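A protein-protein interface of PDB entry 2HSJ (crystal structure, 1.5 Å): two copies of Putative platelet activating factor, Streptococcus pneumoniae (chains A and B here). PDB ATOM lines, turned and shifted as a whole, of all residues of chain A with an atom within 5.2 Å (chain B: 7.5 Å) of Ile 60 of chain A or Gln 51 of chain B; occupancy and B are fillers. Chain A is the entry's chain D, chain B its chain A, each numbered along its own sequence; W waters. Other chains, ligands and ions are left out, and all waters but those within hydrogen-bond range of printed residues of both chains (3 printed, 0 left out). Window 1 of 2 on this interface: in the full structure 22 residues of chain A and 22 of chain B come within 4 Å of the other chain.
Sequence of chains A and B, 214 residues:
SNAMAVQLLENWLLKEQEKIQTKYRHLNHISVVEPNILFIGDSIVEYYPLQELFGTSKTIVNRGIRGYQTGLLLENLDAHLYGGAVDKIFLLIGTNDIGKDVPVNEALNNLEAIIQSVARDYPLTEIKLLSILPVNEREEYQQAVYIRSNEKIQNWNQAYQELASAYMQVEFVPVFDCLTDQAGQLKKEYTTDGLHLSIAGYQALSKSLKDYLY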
ATOM      1  N   VAL A  32      32.297  17.543  -7.533  1.00  0.00           N
ATOM      2  CA  VAL A  32      31.545  18.114  -6.421  1.00  0.00           C
ATOM      3  C   VAL A  32      30.316  17.265  -6.066  1.00  0.00           C
ATOM      4  O   VAL A  32      29.560  17.644  -5.161  1.00  0.00           O
ATOM      5  CB  VAL A  32      31.139  19.594  -6.656  1.00  0.00           C
ATOM      6  CG1 VAL A  32      32.349  20.421  -6.967  1.00  0.00           C
ATOM      7  CG2 VAL A  32      30.075  19.720  -7.762  1.00  0.00           C
ATOM      8  N   VAL A  33      30.108  16.140  -6.754  1.00  0.00           N
ATOM      9  CA  VAL A  33      28.965  15.286  -6.431  1.00  0.00           C
ATOM     10  C   VAL A  33      29.454  13.965  -5.851  1.00  0.00           C
ATOM     11  O   VAL A  33      30.588  13.542  -6.087  1.00  0.00           O
ATOM     12  CB  VAL A  33      28.039  15.032  -7.652  1.00  0.00           C
ATOM     13  CG1 VAL A  33      27.522  16.359  -8.180  1.00  0.00           C
ATOM     14  CG2 VAL A  33      28.776  14.267  -8.762  1.00  0.00           C
ATOM     15  N   ASN A  36      25.864   8.107  -6.394  1.00  0.00           N
ATOM     16  CA  ASN A  36      25.089   7.039  -5.786  1.00  0.00           C
ATOM     17  C   ASN A  36      25.194   5.785  -6.648  1.00  0.00           C
ATOM     18  O   ASN A  36      25.271   4.658  -6.134  1.00  0.00           O
ATOM     19  CB  ASN A  36      23.640   7.487  -5.591  1.00  0.00           C
ATOM     20  CG  ASN A  36      22.774   6.398  -4.985  1.00  0.00           C
ATOM     21  OD1 ASN A  36      22.042   5.707  -5.708  1.00  0.00           O
ATOM     22  ND2 ASN A  36      22.878   6.203  -3.646  1.00  0.00           N
ATOM     23  N   ILE A  37      25.199   5.994  -7.970  1.00  0.00           N
ATOM     24  CA  ILE A  37      25.346   4.922  -8.939  1.00  0.00           C
ATOM     25  C   ILE A  37      26.475   5.360  -9.877  1.00  0.00           C
ATOM     26  O   ILE A  37      26.501   6.527 -10.329  1.00  0.00           O
ATOM     27  CB  ILE A  37      24.035   4.737  -9.774  1.00  0.00           C
ATOM     28  CG1 ILE A  37      22.801   4.659  -8.857  1.00  0.00           C
ATOM     29  CG2 ILE A  37      24.164   3.602 -10.790  1.00  0.00           C
ATOM     30  CD1 ILE A  37      22.619   3.427  -8.093  1.00  0.00           C
ATOM     31  N   PHE A  39      27.817   4.343 -13.581  1.00  0.00           N
ATOM     32  CA  PHE A  39      27.587   3.540 -14.790  1.00  0.00           C
ATOM     33  C   PHE A  39      28.930   3.403 -15.479  1.00  0.00           C
ATOM     34  O   PHE A  39      29.554   4.405 -15.826  1.00  0.00           O
ATOM     35  CB  PHE A  39      26.587   4.224 -15.738  1.00  0.00           C
ATOM     36  CG  PHE A  39      25.175   3.698 -15.629  1.00  0.00           C
ATOM     37  CD1 PHE A  39      24.428   3.929 -14.487  1.00  0.00           C
ATOM     38  CD2 PHE A  39      24.600   2.985 -16.676  1.00  0.00           C
ATOM     39  CE1 PHE A  39      23.118   3.463 -14.377  1.00  0.00           C
ATOM     40  CE2 PHE A  39      23.294   2.497 -16.561  1.00  0.00           C
ATOM     41  CZ  PHE A  39      22.563   2.739 -15.419  1.00  0.00           C
ATOM     42  N   LEU A  50      21.901   9.799 -19.351  1.00  0.00           N
ATOM     43  CA  LEU A  50      21.417   9.386 -18.032  1.00  0.00           C
ATOM     44  C   LEU A  50      20.531  10.407 -17.324  1.00  0.00           C
ATOM     45  O   LEU A  50      19.493  10.058 -16.769  1.00  0.00           O
ATOM     46  CB  LEU A  50      22.609   9.043 -17.149  1.00  0.00           C
ATOM     47  CG  LEU A  50      23.427   7.864 -17.628  1.00  0.00           C
ATOM     48  CD1 LEU A  50      24.814   7.841 -16.930  1.00  0.00           C
ATOM     49  CD2 LEU A  50      22.702   6.578 -17.372  1.00  0.00           C
ATOM     50  N   PHE A  54      16.783   9.285 -16.649  1.00  0.00           N
ATOM     51  CA  PHE A  54      16.521   8.850 -15.257  1.00  0.00           C
ATOM     52  C   PHE A  54      16.159   9.995 -14.303  1.00  0.00           C
ATOM     53  O   PHE A  54      15.580   9.773 -13.240  1.00  0.00           O
ATOM     54  CB  PHE A  54      17.739   8.118 -14.692  1.00  0.00           C
ATOM     55  CG  PHE A  54      17.973   6.745 -15.279  1.00  0.00           C
ATOM     56  CD1 PHE A  54      17.029   5.720 -15.097  1.00  0.00           C
ATOM     57  CD2 PHE A  54      19.143   6.477 -15.975  1.00  0.00           C
ATOM     58  CE1 PHE A  54      17.266   4.455 -15.624  1.00  0.00           C
ATOM     59  CE2 PHE A  54      19.412   5.227 -16.510  1.00  0.00           C
ATOM     60  CZ  PHE A  54      18.467   4.192 -16.328  1.00  0.00           C
ATOM     61  N   LYS A  58      18.417  10.944  -8.083  1.00  0.00           N
ATOM     62  CA  LYS A  58      19.433   9.957  -7.747  1.00  0.00           C
ATOM     63  C   LYS A  58      20.631  10.324  -8.612  1.00  0.00           C
ATOM     64  O   LYS A  58      20.506  10.414  -9.852  1.00  0.00           O
ATOM     65  CB  LYS A  58      18.922   8.555  -8.113  1.00  0.00           C
ATOM     66  CG  LYS A  58      19.890   7.435  -7.841  1.00  0.00           C
ATOM     67  CD  LYS A  58      19.210   6.078  -8.033  1.00  0.00           C
ATOM     68  CE  LYS A  58      18.390   5.646  -6.836  1.00  0.00           C
ATOM     69  NZ  LYS A  58      19.218   4.895  -5.854  1.00  0.00           N
ATOM     70  N   THR A  59      21.796  10.500  -7.988  1.00  0.00           N
ATOM     71  CA  THR A  59      22.989  10.919  -8.714  1.00  0.00           C
ATOM     72  C   THR A  59      23.691   9.739  -9.357  1.00  0.00           C
ATOM     73  O   THR A  59      24.306   8.900  -8.672  1.00  0.00           O
ATOM     74  CB  THR A  59      23.988  11.677  -7.827  1.00  0.00           C
ATOM     75  OG1 THR A  59      23.300  12.776  -7.218  1.00  0.00           O
ATOM     76  CG2 THR A  59      25.142  12.227  -8.645  1.00  0.00           C
ATOM     77  N   ILE A  60      23.611   9.707 -10.687  1.00  0.00           N
ATOM     78  CA  ILE A  60      24.198   8.648 -11.495  1.00  0.00           C
ATOM     79  C   ILE A  60      25.290   9.322 -12.307  1.00  0.00           C
ATOM     80  O   ILE A  60      25.061  10.310 -12.988  1.00  0.00           O
ATOM     81  CB  ILE A  60      23.158   8.059 -12.488  1.00  0.00           C
ATOM     82  CG1 ILE A  60      21.910   7.639 -11.688  1.00  0.00           C
ATOM     83  CG2 ILE A  60      23.808   6.890 -13.294  1.00  0.00           C
ATOM     84  CD1 ILE A  60      20.729   7.031 -12.522  1.00  0.00           C
ATOM     85  N   VAL A  61      26.491   8.773 -12.187  1.00  0.00           N
ATOM     86  CA  VAL A  61      27.653   9.359 -12.855  1.00  0.00           C
ATOM     87  C   VAL A  61      28.160   8.453 -13.968  1.00  0.00           C
ATOM     88  O   VAL A  61      28.289   7.235 -13.793  1.00  0.00           O
ATOM     89  CB  VAL A  61      28.798   9.692 -11.817  1.00  0.00           C
ATOM     90  CG1 VAL A  61      30.092  10.138 -12.475  1.00  0.00           C
ATOM     91  CG2 VAL A  61      28.348  10.778 -10.851  1.00  0.00           C
ATOM     92  N   ASN A  62      28.483   9.070 -15.107  1.00  0.00           N
ATOM     93  CA  ASN A  62      28.906   8.335 -16.290  1.00  0.00           C
ATOM     94  C   ASN A  62      30.402   8.095 -16.231  1.00  0.00           C
ATOM     95  O   ASN A  62      31.207   9.041 -16.201  1.00  0.00           O
ATOM     96  CB  ASN A  62      28.587   9.166 -17.526  1.00  0.00           C
ATOM     97  CG  ASN A  62      28.518   8.317 -18.769  1.00  0.00           C
ATOM     98  OD1 ASN A  62      29.398   7.505 -19.016  1.00  0.00           O
ATOM     99  ND2 ASN A  62      27.440   8.473 -19.553  1.00  0.00           N
ATOM    100  N   LEU A 213      17.826   0.309  -9.924  1.00  0.00           N
ATOM    101  CA  LEU A 213      18.505   1.452  -9.307  1.00  0.00           C
ATOM    102  C   LEU A 213      18.330   1.511  -7.780  1.00  0.00           C
ATOM    103  O   LEU A 213      19.075   2.247  -7.100  1.00  0.00           O
ATOM    104  CB  LEU A 213      17.978   2.761  -9.891  1.00  0.00           C
ATOM    105  CG  LEU A 213      18.323   3.014 -11.354  1.00  0.00           C
ATOM    106  CD1 LEU A 213      17.530   4.230 -11.788  1.00  0.00           C
ATOM    107  CD2 LEU A 213      19.797   3.239 -11.555  1.00  0.00           C
ATOM    108  N   TYR B  48      31.847  19.584 -21.700  1.00  0.00           N
ATOM    109  CA  TYR B  48      31.883  20.175 -20.350  1.00  0.00           C
ATOM    110  C   TYR B  48      31.269  19.215 -19.336  1.00  0.00           C
ATOM    111  O   TYR B  48      30.122  18.781 -19.508  1.00  0.00           O
ATOM    112  CB  TYR B  48      31.016  21.421 -20.367  1.00  0.00           C
ATOM    113  CG  TYR B  48      31.327  22.488 -19.330  1.00  0.00           C
ATOM    114  CD1 TYR B  48      31.349  23.834 -19.703  1.00  0.00           C
ATOM    115  CD2 TYR B  48      31.563  22.175 -17.976  1.00  0.00           C
ATOM    116  CE1 TYR B  48      31.596  24.837 -18.772  1.00  0.00           C
ATOM    117  CE2 TYR B  48      31.854  23.180 -17.024  1.00  0.00           C
ATOM    118  CZ  TYR B  48      31.869  24.514 -17.436  1.00  0.00           C
ATOM    119  OH  TYR B  48      32.135  25.547 -16.547  1.00  0.00           O
ATOM    120  N   PRO B  49      32.025  18.840 -18.294  1.00  0.00           N
ATOM    121  CA  PRO B  49      31.492  17.988 -17.221  1.00  0.00           C
ATOM    122  C   PRO B  49      30.629  18.788 -16.251  1.00  0.00           C
ATOM    123  O   PRO B  49      31.005  19.081 -15.102  1.00  0.00           O
ATOM    124  CB  PRO B  49      32.745  17.420 -16.521  1.00  0.00           C
ATOM    125  CG  PRO B  49      33.863  18.331 -16.880  1.00  0.00           C
ATOM    126  CD  PRO B  49      33.462  19.123 -18.133  1.00  0.00           C
ATOM    127  N   LEU B  50      29.446  19.178 -16.753  1.00  0.00           N
ATOM    128  CA  LEU B  50      28.539  20.054 -15.986  1.00  0.00           C
ATOM    129  C   LEU B  50      28.124  19.471 -14.641  1.00  0.00           C
ATOM    130  O   LEU B  50      28.202  20.159 -13.623  1.00  0.00           O
ATOM    131  CB  LEU B  50      27.272  20.371 -16.803  1.00  0.00           C
ATOM    132  CG  LEU B  50      27.557  21.131 -18.100  1.00  0.00           C
ATOM    133  CD1 LEU B  50      26.287  21.154 -18.978  1.00  0.00           C
ATOM    134  CD2 LEU B  50      28.032  22.539 -17.816  1.00  0.00           C
ATOM    135  N   GLN B  51      27.715  18.205 -14.645  1.00  0.00           N
ATOM    136  CA  GLN B  51      27.249  17.583 -13.406  1.00  0.00           C
ATOM    137  C   GLN B  51      28.346  17.583 -12.345  1.00  0.00           C
ATOM    138  O   GLN B  51      28.120  17.933 -11.192  1.00  0.00           O
ATOM    139  CB  GLN B  51      26.859  16.132 -13.662  1.00  0.00           C
ATOM    140  CG  GLN B  51      26.319  15.387 -12.450  1.00  0.00           C
ATOM    141  CD  GLN B  51      26.407  13.895 -12.687  1.00  0.00           C
ATOM    142  OE1 GLN B  51      27.421  13.396 -13.180  1.00  0.00           O
ATOM    143  NE2 GLN B  51      25.342  13.175 -12.365  1.00  0.00           N
ATOM    144  N   GLU B  52      29.510  17.083 -12.730  1.00  0.00           N
ATOM    145  CA  GLU B  52      30.555  16.866 -11.721  1.00  0.00           C
ATOM    146  C   GLU B  52      31.251  18.159 -11.290  1.00  0.00           C
ATOM    147  O   GLU B  52      31.847  18.196 -10.217  1.00  0.00           O
ATOM    148  CB  GLU B  52      31.566  15.791 -12.200  1.00  0.00           C
ATOM    149  CG  GLU B  52      30.920  14.423 -12.366  1.00  0.00           C
ATOM    150  CD  GLU B  52      31.940  13.344 -12.715  1.00  0.00           C
ATOM    151  OE1 GLU B  52      32.596  12.816 -11.777  1.00  0.00           O
ATOM    152  OE2 GLU B  52      32.121  13.105 -13.939  1.00  0.00           O
ATOM    153  N   LEU B  53      31.135  19.215 -12.101  1.00  0.00           N
ATOM    154  CA  LEU B  53      31.762  20.484 -11.686  1.00  0.00           C
ATOM    155  C   LEU B  53      30.842  21.526 -11.071  1.00  0.00           C
ATOM    156  O   LEU B  53      31.336  22.347 -10.251  1.00  0.00           O
ATOM    157  CB  LEU B  53      32.594  21.107 -12.811  1.00  0.00           C
ATOM    158  CG  LEU B  53      33.763  20.220 -13.240  1.00  0.00           C
ATOM    159  CD1 LEU B  53      34.490  20.872 -14.411  1.00  0.00           C
ATOM    160  CD2 LEU B  53      34.773  19.964 -12.109  1.00  0.00           C
ATOM    161  N   PHE B  54      29.554  21.543 -11.501  1.00  0.00           N
ATOM    162  CA  PHE B  54      28.565  22.470 -10.929  1.00  0.00           C
ATOM    163  C   PHE B  54      27.644  21.813  -9.898  1.00  0.00           C
ATOM    164  O   PHE B  54      26.984  22.506  -9.096  1.00  0.00           O
ATOM    165  CB  PHE B  54      27.705  23.081 -12.021  1.00  0.00           C
ATOM    166  CG  PHE B  54      28.408  24.105 -12.859  1.00  0.00           C
ATOM    167  CD1 PHE B  54      28.997  25.228 -12.270  1.00  0.00           C
ATOM    168  CD2 PHE B  54      28.469  23.954 -14.247  1.00  0.00           C
ATOM    169  CE1 PHE B  54      29.624  26.212 -13.058  1.00  0.00           C
ATOM    170  CE2 PHE B  54      29.116  24.914 -15.041  1.00  0.00           C
ATOM    171  CZ  PHE B  54      29.682  26.054 -14.439  1.00  0.00           C
ATOM    172  N   GLY B  55      27.538  20.486  -9.944  1.00  0.00           N
ATOM    173  CA  GLY B  55      26.607  19.803  -9.062  1.00  0.00           C
ATOM    174  C   GLY B  55      25.195  19.909  -9.608  1.00  0.00           C
ATOM    175  O   GLY B  55      24.984  20.387 -10.733  1.00  0.00           O
ATOM    176  N   THR B  56      24.220  19.455  -8.814  1.00  0.00           N
ATOM    177  CA  THR B  56      22.883  19.260  -9.347  1.00  0.00           C
ATOM    178  C   THR B  56      21.828  20.012  -8.537  1.00  0.00           C
ATOM    179  O   THR B  56      20.630  19.724  -8.657  1.00  0.00           O
ATOM    180  CB  THR B  56      22.532  17.765  -9.445  1.00  0.00           C
ATOM    181  OG1 THR B  56      22.526  17.201  -8.136  1.00  0.00           O
ATOM    182  CG2 THR B  56      23.582  17.021 -10.298  1.00  0.00           C
ATOM    183  N   SER B  57      22.254  21.018  -7.769  1.00  0.00           N
ATOM    184  CA  SER B  57      21.269  21.832  -7.030  1.00  0.00           C
ATOM    185  C   SER B  57      20.266  22.454  -8.019  1.00  0.00           C
ATOM    186  O   SER B  57      19.094  22.614  -7.698  1.00  0.00           O
ATOM    187  CB  SER B  57      21.943  22.915  -6.184  1.00  0.00           C
ATOM    188  OG  SER B  57      22.547  23.911  -6.983  1.00  0.00           O
ATOM    189  N   ILE B  60      20.915  21.410 -14.879  1.00  0.00           N
ATOM    190  CA  ILE B  60      21.659  22.013 -15.996  1.00  0.00           C
ATOM    191  C   ILE B  60      21.764  20.957 -17.090  1.00  0.00           C
ATOM    192  O   ILE B  60      22.267  19.858 -16.862  1.00  0.00           O
ATOM    193  CB  ILE B  60      23.096  22.453 -15.576  1.00  0.00           C
ATOM    194  CG1 ILE B  60      23.055  23.334 -14.316  1.00  0.00           C
ATOM    195  CG2 ILE B  60      23.820  23.160 -16.766  1.00  0.00           C
ATOM    196  CD1 ILE B  60      24.461  23.674 -13.835  1.00  0.00           C
ATOM    197  N   ASN B  62      22.912  19.800 -21.021  1.00  0.00           N
ATOM    198  CA  ASN B  62      23.902  20.021 -22.083  1.00  0.00           C
ATOM    199  C   ASN B  62      23.235  19.927 -23.459  1.00  0.00           C
ATOM    200  O   ASN B  62      22.606  18.902 -23.810  1.00  0.00           O
ATOM    201  CB  ASN B  62      24.978  18.956 -21.969  1.00  0.00           C
ATOM    202  CG  ASN B  62      26.261  19.330 -22.706  1.00  0.00           C
ATOM    203  OD1 ASN B  62      26.217  19.816 -23.825  1.00  0.00           O
ATOM    204  ND2 ASN B  62      27.415  19.158 -22.041  1.00  0.00           N
HETATM  205  O   HOH W   1      21.913  14.368  -9.063  1.00  0.00           O
HETATM  206  O   HOH W   2      28.318  11.983 -15.273  1.00  0.00           O
HETATM  207  O   HOH W   3      24.388  15.391  -6.497  1.00  0.00           O
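The side-chain amide nitrogen (NE2) of Gln 51 of chain B sits at hydrogen-bond distance from the backbone carbonyl oxygen (O) of Ile 60 of chain A, at 2.9 Å. The backbone carbonyl oxygen (O) of Glu 52 of chain B is in hydrogen-bond range of the backbone NH (N) of Val 32 of chain A, 2.8 Å away.
The backbone NH (N) of Asn 36 of chain A is in hydrogen-bond range of the backbone carbonyl oxygen (O) of Thr 59 of chain A, 2.9 Å away. The backbone NH of Ile 37 of chain A sits at hydrogen-bond distance from the backbone carbonyl oxygen of Thr 59 of chain A (3.1 Å). The backbone carbonyl oxygen of Ile 37 of chain A is in hydrogen-bond range of the backbone NH of Val 61 of chain A (2.9 Å). N of Phe 39 of chain A sits at hydrogen-bond distance from O of Val 61 of chain A.
CG2 of Val 32 of chain A touches O of Leu 53 of chain B (3.8 Å). Phe 54 of chain B touches Val 32 of chain A (C to CG2, 3.9 Å). Gly 55 of chain B touches Val 32 of chain A (N to CG2, 3.4 Å). Val 33 of chain A touches Gln 51 of chain B. CG1 of Val 33 of chain A touches CA of Gly 55 of chain B (3.7 Å). Gln 51 of chain B touches Thr 59 of chain A (NE2 to CG2, 3.8 Å). OE1 of Gln 51 of chain B touches CG2 of Val 61 of chain A, at 3.6 Å. Val 61 of chain A touches Glu 52 of chain B (CG1 to CD, 3.7 Å).
Ile 60 of chain A touches just one residue of chain B: Gln 51 (2.9 Å). Gln 51 of chain B touches just these residues of chain A: Val 33 (3.5 Å), Thr 59 (3.8 Å), Ile 60 (2.9 Å) and Val 61 (3.6 Å). Of the printed residues of chain A, Leu 53 of chain B touches Val 32 (3.8 Å). Printed residues of chain A within 4 Å of Phe 54 of chain B: Val 32 (3.9 Å). Pro 49 of chain B touches none of the printed residues of chain A. The nearest residue of chain B that does not touch Ile 60 of chain A is Glu 52 of chain B (7.2 Å). The nearest printed residue of chain A that does not touch Phe 54 of chain B is Val 33 of chain A (5.7 Å).
Of the 13 printed residues of chain A, 5 touch a printed residue of chain B. Among the printed residues, no Asp or Glu carboxylate lies within 4 Å of a Lys or Arg side-chain nitrogen of the other chain.
Positions printed for both chains: 50, 54, 60 and 62.
Water W2 lies within hydrogen-bond range of OE1 of Gln 51 of chain B (2.7 Å) and N of Asn 62 of chain A (2.9 Å). Water W1 lies within hydrogen-bond range of the side-chain hydroxyl (OG1) of Thr 59 of chain A (2.8 Å) and the side-chain hydroxyl (OG1) of Thr 56 of chain B (3.0 Å). Water W3 bridges the side-chain hydroxyl (OG1) of Thr 59 of chain A (2.9 Å) and the side-chain hydroxyl (OG1) of Thr 56 of chain B (3.1 Å).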
